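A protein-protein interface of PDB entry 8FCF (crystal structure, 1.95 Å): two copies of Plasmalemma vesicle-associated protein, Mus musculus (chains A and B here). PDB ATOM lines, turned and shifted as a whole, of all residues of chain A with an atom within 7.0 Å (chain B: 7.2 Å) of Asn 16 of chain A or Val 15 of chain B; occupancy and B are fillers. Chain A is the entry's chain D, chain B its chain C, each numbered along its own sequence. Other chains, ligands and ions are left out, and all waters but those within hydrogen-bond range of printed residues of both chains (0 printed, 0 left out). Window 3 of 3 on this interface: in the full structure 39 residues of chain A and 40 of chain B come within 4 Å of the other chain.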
ATOM      1  N   LEU A  12     -17.985  -1.307  20.156  1.00  0.00           N
ATOM      2  CA  LEU A  12     -18.340  -0.362  19.088  1.00  0.00           C
ATOM      3  C   LEU A  12     -17.971   1.089  19.500  1.00  0.00           C
ATOM      4  O   LEU A  12     -17.789   1.966  18.632  1.00  0.00           O
ATOM      5  CB  LEU A  12     -19.813  -0.499  18.676  1.00  0.00           C
ATOM      6  CG  LEU A  12     -20.365  -1.954  18.548  1.00  0.00           C
ATOM      7  CD1 LEU A  12     -21.848  -2.025  18.933  1.00  0.00           C
ATOM      8  CD2 LEU A  12     -20.118  -2.532  17.134  1.00  0.00           C
ATOM      9  N   LYS A  13     -17.797   1.329  20.836  1.00  0.00           N
ATOM     10  CA  LYS A  13     -17.177   2.560  21.347  1.00  0.00           C
ATOM     11  C   LYS A  13     -15.695   2.435  20.937  1.00  0.00           C
ATOM     12  O   LYS A  13     -15.043   3.427  20.637  1.00  0.00           O
ATOM     13  CB  LYS A  13     -17.238   2.652  22.893  1.00  0.00           C
ATOM     14  CG  LYS A  13     -16.571   3.946  23.464  1.00  0.00           C
ATOM     15  CD  LYS A  13     -17.409   4.666  24.554  1.00  0.00           C
ATOM     16  CE  LYS A  13     -18.641   5.401  24.015  1.00  0.00           C
ATOM     17  NZ  LYS A  13     -19.829   4.528  23.769  1.00  0.00           N
ATOM     18  N   GLU A  14     -15.192   1.175  20.930  1.00  0.00           N
ATOM     19  CA  GLU A  14     -13.833   0.787  20.546  1.00  0.00           C
ATOM     20  C   GLU A  14     -13.446   1.340  19.165  1.00  0.00           C
ATOM     21  O   GLU A  14     -12.380   1.937  19.039  1.00  0.00           O
ATOM     22  CB  GLU A  14     -13.699  -0.754  20.534  1.00  0.00           C
ATOM     23  CG  GLU A  14     -13.772  -1.425  21.902  1.00  0.00           C
ATOM     24  CD  GLU A  14     -13.962  -2.936  21.849  1.00  0.00           C
ATOM     25  OE1 GLU A  14     -13.038  -3.637  21.374  1.00  0.00           O
ATOM     26  OE2 GLU A  14     -15.032  -3.418  22.290  1.00  0.00           O
ATOM     27  N   VAL A  15     -14.310   1.141  18.140  1.00  0.00           N
ATOM     28  CA  VAL A  15     -14.036   1.607  16.768  1.00  0.00           C
ATOM     29  C   VAL A  15     -14.058   3.168  16.688  1.00  0.00           C
ATOM     30  O   VAL A  15     -13.235   3.733  15.948  1.00  0.00           O
ATOM     31  CB  VAL A  15     -14.924   0.908  15.678  1.00  0.00           C
ATOM     32  CG1 VAL A  15     -16.410   1.231  15.829  1.00  0.00           C
ATOM     33  CG2 VAL A  15     -14.439   1.229  14.268  1.00  0.00           C
ATOM     34  N   ASN A  16     -14.926   3.862  17.483  1.00  0.00           N
ATOM     35  CA  ASN A  16     -14.902   5.337  17.476  1.00  0.00           C
ATOM     36  C   ASN A  16     -13.631   5.896  18.161  1.00  0.00           C
ATOM     37  O   ASN A  16     -13.150   6.947  17.756  1.00  0.00           O
ATOM     38  CB  ASN A  16     -16.161   5.958  18.077  1.00  0.00           C
ATOM     39  CG  ASN A  16     -16.504   7.287  17.409  1.00  0.00           C
ATOM     40  OD1 ASN A  16     -16.847   7.333  16.223  1.00  0.00           O
ATOM     41  ND2 ASN A  16     -16.416   8.399  18.126  1.00  0.00           N
ATOM     42  N   LYS A  17     -13.083   5.185  19.165  1.00  0.00           N
ATOM     43  CA  LYS A  17     -11.841   5.586  19.830  1.00  0.00           C
ATOM     44  C   LYS A  17     -10.693   5.524  18.833  1.00  0.00           C
ATOM     45  O   LYS A  17      -9.878   6.441  18.790  1.00  0.00           O
ATOM     46  CB  LYS A  17     -11.515   4.684  21.035  1.00  0.00           C
ATOM     47  CG  LYS A  17     -12.361   4.925  22.263  1.00  0.00           C
ATOM     48  CD  LYS A  17     -11.736   4.238  23.468  1.00  0.00           C
ATOM     49  CE  LYS A  17     -12.681   4.057  24.637  1.00  0.00           C
ATOM     50  NZ  LYS A  17     -11.945   4.054  25.935  1.00  0.00           N
ATOM     51  N   THR A  18     -10.621   4.446  18.033  1.00  0.00           N
ATOM     52  CA  THR A  18      -9.553   4.324  17.027  1.00  0.00           C
ATOM     53  C   THR A  18      -9.660   5.395  15.933  1.00  0.00           C
ATOM     54  O   THR A  18      -8.618   5.837  15.420  1.00  0.00           O
ATOM     55  CB  THR A  18      -9.456   2.903  16.435  1.00  0.00           C
ATOM     56  OG1 THR A  18     -10.566   2.625  15.580  1.00  0.00           O
ATOM     57  CG2 THR A  18      -9.303   1.847  17.492  1.00  0.00           C
ATOM     58  N   CYS A  19     -10.904   5.800  15.562  1.00  0.00           N
ATOM     59  CA  CYS A  19     -11.113   6.861  14.580  1.00  0.00           C
ATOM     60  C   CYS A  19     -10.593   8.201  15.118  1.00  0.00           C
ATOM     61  O   CYS A  19      -9.882   8.893  14.414  1.00  0.00           O
ATOM     62  CB  CYS A  19     -12.582   6.968  14.177  1.00  0.00           C
ATOM     63  SG  CYS A  19     -12.946   8.413  13.129  1.00  0.00           S
ATOM     64  N   GLU A  20     -10.975   8.568  16.347  1.00  0.00           N
ATOM     65  CA  GLU A  20     -10.542   9.806  17.003  1.00  0.00           C
ATOM     66  C   GLU A  20      -9.031   9.867  17.230  1.00  0.00           C
ATOM     67  O   GLU A  20      -8.429  10.911  16.990  1.00  0.00           O
ATOM     68  CB  GLU A  20     -11.339   9.990  18.294  1.00  0.00           C
ATOM     69  CG  GLU A  20     -12.797  10.278  17.972  1.00  0.00           C
ATOM     70  CD  GLU A  20     -13.757  10.293  19.146  1.00  0.00           C
ATOM     71  OE1 GLU A  20     -13.323   9.990  20.281  1.00  0.00           O
ATOM     72  OE2 GLU A  20     -14.950  10.608  18.928  1.00  0.00           O
ATOM     73  N   ALA A  21      -8.401   8.756  17.609  1.00  0.00           N
ATOM     74  CA  ALA A  21      -6.946   8.693  17.759  1.00  0.00           C
ATOM     75  C   ALA A  21      -6.253   8.905  16.387  1.00  0.00           C
ATOM     76  O   ALA A  21      -5.194   9.522  16.325  1.00  0.00           O
ATOM     77  CB  ALA A  21      -6.539   7.352  18.348  1.00  0.00           C
ATOM     78  N   LEU A  22      -6.875   8.425  15.294  1.00  0.00           N
ATOM     79  CA  LEU A  22      -6.324   8.596  13.946  1.00  0.00           C
ATOM     80  C   LEU A  22      -6.483  10.039  13.479  1.00  0.00           C
ATOM     81  O   LEU A  22      -5.662  10.490  12.708  1.00  0.00           O
ATOM     82  CB  LEU A  22      -6.996   7.656  12.907  1.00  0.00           C
ATOM     83  CG  LEU A  22      -6.129   6.586  12.220  1.00  0.00           C
ATOM     84  CD1 LEU A  22      -6.911   5.898  11.081  1.00  0.00           C
ATOM     85  CD2 LEU A  22      -4.844   7.179  11.655  1.00  0.00           C
ATOM     86  N   GLU B  10     -28.296   1.695  16.085  1.00  0.00           N
ATOM     87  CA  GLU B  10     -28.394   2.837  15.157  1.00  0.00           C
ATOM     88  C   GLU B  10     -27.659   4.080  15.684  1.00  0.00           C
ATOM     89  O   GLU B  10     -27.188   4.872  14.867  1.00  0.00           O
ATOM     90  CB  GLU B  10     -29.871   3.166  14.789  1.00  0.00           C
ATOM     91  CG  GLU B  10     -30.626   4.171  15.667  1.00  0.00           C
ATOM     92  CD  GLU B  10     -31.006   3.765  17.086  1.00  0.00           C
ATOM     93  OE1 GLU B  10     -30.793   2.586  17.458  1.00  0.00           O
ATOM     94  OE2 GLU B  10     -31.544   4.629  17.820  1.00  0.00           O
ATOM     95  N   GLN B  11     -27.564   4.263  17.025  1.00  0.00           N
ATOM     96  CA  GLN B  11     -26.892   5.443  17.588  1.00  0.00           C
ATOM     97  C   GLN B  11     -25.376   5.375  17.436  1.00  0.00           C
ATOM     98  O   GLN B  11     -24.760   6.342  16.983  1.00  0.00           O
ATOM     99  CB  GLN B  11     -27.288   5.660  19.060  1.00  0.00           C
ATOM    100  CG  GLN B  11     -26.859   7.022  19.654  1.00  0.00           C
ATOM    101  CD  GLN B  11     -27.345   8.244  18.899  1.00  0.00           C
ATOM    102  OE1 GLN B  11     -26.809   8.620  17.848  1.00  0.00           O
ATOM    103  NE2 GLN B  11     -28.346   8.933  19.442  1.00  0.00           N
ATOM    104  N   LEU B  12     -24.778   4.238  17.809  1.00  0.00           N
ATOM    105  CA  LEU B  12     -23.331   4.039  17.684  1.00  0.00           C
ATOM    106  C   LEU B  12     -22.870   4.006  16.215  1.00  0.00           C
ATOM    107  O   LEU B  12     -21.719   4.338  15.949  1.00  0.00           O
ATOM    108  CB  LEU B  12     -22.874   2.763  18.439  1.00  0.00           C
ATOM    109  CG  LEU B  12     -22.267   2.952  19.847  1.00  0.00           C
ATOM    110  CD1 LEU B  12     -22.964   4.067  20.643  1.00  0.00           C
ATOM    111  CD2 LEU B  12     -22.339   1.658  20.643  1.00  0.00           C
ATOM    112  N   LYS B  13     -23.757   3.634  15.274  1.00  0.00           N
ATOM    113  CA  LYS B  13     -23.428   3.624  13.849  1.00  0.00           C
ATOM    114  C   LYS B  13     -23.440   5.048  13.302  1.00  0.00           C
ATOM    115  O   LYS B  13     -22.574   5.384  12.503  1.00  0.00           O
ATOM    116  CB  LYS B  13     -24.406   2.739  13.054  1.00  0.00           C
ATOM    117  CG  LYS B  13     -24.257   1.247  13.349  1.00  0.00           C
ATOM    118  CD  LYS B  13     -23.247   0.543  12.457  1.00  0.00           C
ATOM    119  CE  LYS B  13     -23.211  -0.941  12.752  1.00  0.00           C
ATOM    120  NZ  LYS B  13     -22.085  -1.628  12.062  1.00  0.00           N
ATOM    121  N   GLU B  14     -24.416   5.882  13.729  1.00  0.00           N
ATOM    122  CA  GLU B  14     -24.537   7.282  13.292  1.00  0.00           C
ATOM    123  C   GLU B  14     -23.352   8.139  13.789  1.00  0.00           C
ATOM    124  O   GLU B  14     -22.854   8.977  13.044  1.00  0.00           O
ATOM    125  CB  GLU B  14     -25.874   7.883  13.768  1.00  0.00           C
ATOM    126  CG  GLU B  14     -26.178   9.273  13.214  1.00  0.00           C
ATOM    127  CD  GLU B  14     -27.439   9.392  12.381  1.00  0.00           C
ATOM    128  OE1 GLU B  14     -27.331   9.777  11.194  1.00  0.00           O
ATOM    129  OE2 GLU B  14     -28.536   9.110  12.915  1.00  0.00           O
ATOM    130  N   VAL B  15     -22.924   7.932  15.044  1.00  0.00           N
ATOM    131  CA  VAL B  15     -21.780   8.620  15.672  1.00  0.00           C
ATOM    132  C   VAL B  15     -20.501   8.316  14.875  1.00  0.00           C
ATOM    133  O   VAL B  15     -19.689   9.204  14.586  1.00  0.00           O
ATOM    134  CB  VAL B  15     -21.649   8.137  17.151  1.00  0.00           C
ATOM    135  CG1 VAL B  15     -20.281   8.458  17.745  1.00  0.00           C
ATOM    136  CG2 VAL B  15     -22.756   8.728  18.019  1.00  0.00           C
ATOM    137  N   ASN B  16     -20.314   7.040  14.551  1.00  0.00           N
ATOM    138  CA  ASN B  16     -19.138   6.575  13.839  1.00  0.00           C
ATOM    139  C   ASN B  16     -19.116   6.997  12.368  1.00  0.00           C
ATOM    140  O   ASN B  16     -18.051   7.307  11.871  1.00  0.00           O
ATOM    141  CB  ASN B  16     -19.002   5.069  14.012  1.00  0.00           C
ATOM    142  CG  ASN B  16     -17.731   4.524  13.458  1.00  0.00           C
ATOM    143  OD1 ASN B  16     -17.751   3.736  12.525  1.00  0.00           O
ATOM    144  ND2 ASN B  16     -16.596   4.929  14.011  1.00  0.00           N
ATOM    145  N   LYS B  17     -20.269   7.067  11.693  1.00  0.00           N
ATOM    146  CA  LYS B  17     -20.360   7.519  10.292  1.00  0.00           C
ATOM    147  C   LYS B  17     -19.768   8.941  10.159  1.00  0.00           C
ATOM    148  O   LYS B  17     -19.053   9.248   9.196  1.00  0.00           O
ATOM    149  CB  LYS B  17     -21.845   7.482   9.847  1.00  0.00           C
ATOM    150  CG  LYS B  17     -22.168   8.003   8.444  1.00  0.00           C
ATOM    151  CD  LYS B  17     -23.671   8.331   8.318  1.00  0.00           C
ATOM    152  CE  LYS B  17     -24.265   8.033   6.960  1.00  0.00           C
ATOM    153  NZ  LYS B  17     -23.730   8.901   5.882  1.00  0.00           N
ATOM    154  N   THR B  18     -20.068   9.792  11.135  1.00  0.00           N
ATOM    155  CA  THR B  18     -19.582  11.168  11.213  1.00  0.00           C
ATOM    156  C   THR B  18     -18.059  11.243  11.403  1.00  0.00           C
ATOM    157  O   THR B  18     -17.404  12.018  10.715  1.00  0.00           O
ATOM    158  CB  THR B  18     -20.374  11.892  12.331  1.00  0.00           C
ATOM    159  OG1 THR B  18     -21.719  11.987  11.883  1.00  0.00           O
ATOM    160  CG2 THR B  18     -19.840  13.292  12.642  1.00  0.00           C
ATOM    161  N   CYS B  19     -17.502  10.441  12.330  1.00  0.00           N
ATOM    162  CA  CYS B  19     -16.055  10.403  12.602  1.00  0.00           C
ATOM    163  C   CYS B  19     -15.293   9.865  11.386  1.00  0.00           C
ATOM    164  O   CYS B  19     -14.279  10.447  10.980  1.00  0.00           O
ATOM    165  CB  CYS B  19     -15.768   9.576  13.855  1.00  0.00           C
ATOM    166  SG  CYS B  19     -14.034   9.615  14.395  1.00  0.00           S
ATOM    167  N   GLU B  20     -15.784   8.763  10.791  1.00  0.00           N
ATOM    168  CA  GLU B  20     -15.135   8.155   9.618  1.00  0.00           C
ATOM    169  C   GLU B  20     -15.151   9.104   8.412  1.00  0.00           C
ATOM    170  O   GLU B  20     -14.176   9.175   7.691  1.00  0.00           O
ATOM    171  CB  GLU B  20     -15.844   6.839   9.231  1.00  0.00           C
ATOM    172  CG  GLU B  20     -15.803   5.745  10.286  1.00  0.00           C
ATOM    173  CD  GLU B  20     -14.454   5.143  10.594  1.00  0.00           C
ATOM    174  OE1 GLU B  20     -13.607   5.046   9.677  1.00  0.00           O
ATOM    175  OE2 GLU B  20     -14.238   4.768  11.768  1.00  0.00           O
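The side-chain amide nitrogen of Asn 16 of chain B sits at hydrogen-bond distance from the side-chain amide oxygen of Asn 16 of chain A. SG of Cys 19 of chain A forms a disulfide with SG of Cys 19 of chain B. SG of Cys 19 of chain B lies within hydrogen-bond range of N of Glu 20 of chain A, 3.8 Å away. The side-chain sulfur (SG) of Cys 19 of chain A is in hydrogen-bond range of the backbone NH (N) of Glu 20 of chain B, at 3.7 Å.
The side-chain carboxylate (OE2) of Glu 20 of chain B is in hydrogen-bond range of the side-chain amide nitrogen (ND2) of Asn 16 of chain B (3.3 Å). The side-chain amide nitrogen (ND2) of Asn 16 of chain A sits at hydrogen-bond distance from the side-chain carboxylate (OE2) of Glu 20 of chain A.
Leu 12 of chain B touches Leu 12 of chain A. Asn 16 of chain A touches Val 15 of chain B (OD1 to O, 3.8 Å). Cys 19 of chain B touches Asn 16 of chain A.
Of the printed residues of chain B, Leu 12 of chain A touches Leu 12. Asn 16 of chain A touches just these residues of chain B: Val 15, Asn 16 and Cys 19. Lys 17 of chain A touches none of the printed residues of chain B. Thr 18 of chain A touches none of the printed residues of chain B. Of the printed residues of chain B, Cys 19 of chain A touches Cys 19 (2.1 Å) and Glu 20 (3.7 Å). Of the printed residues of chain A, Leu 12 of chain B touches Leu 12 (3.9 Å). Of chain A, only Asn 16 (3.8 Å) comes within 4 Å of Val 15 of chain B. Of the printed residues of chain A, Asn 16 of chain B touches Asn 16 (3.3 Å). Of the printed residues of chain A, Cys 19 of chain B touches Asn 16, Cys 19 and Glu 20. The nearest printed residue of chain B that does not touch Cys 19 of chain A is Asn 16 of chain B (4.5 Å).
Of the 11 printed residues of chain A, 4 touch a printed residue of chain B. Printed residues of chain A that touch a printed residue of chain B: Leu 12, Asn 16, Cys 19 and Glu 20. Hydrophobic or aromatic side chains of chain B within 4 Å of the printed part of chain A: Leu 12 and Val 15. Along chain B the printed residues that touch a printed residue of chain A span positions 12 to 20. Among the printed residues, 7 pairs touch across the chains.
Leu 12 of chain B touches its own counterpart, Leu 12 of chain A. Asn 16 of chain B touches its own counterpart, Asn 16 of chain A. Cys 19 of chain B touches its own counterpart, Cys 19 of chain A. Cys 19 of chain A touches Glu 20 of chain B, and with the chains exchanged Glu 20 of chain A touches Cys 19 of chain B. 9 positions are printed for both chains. Of the 7 pairs that touch across the chains among the printed residues, 5 have their exchanged pair printed and touching as well.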
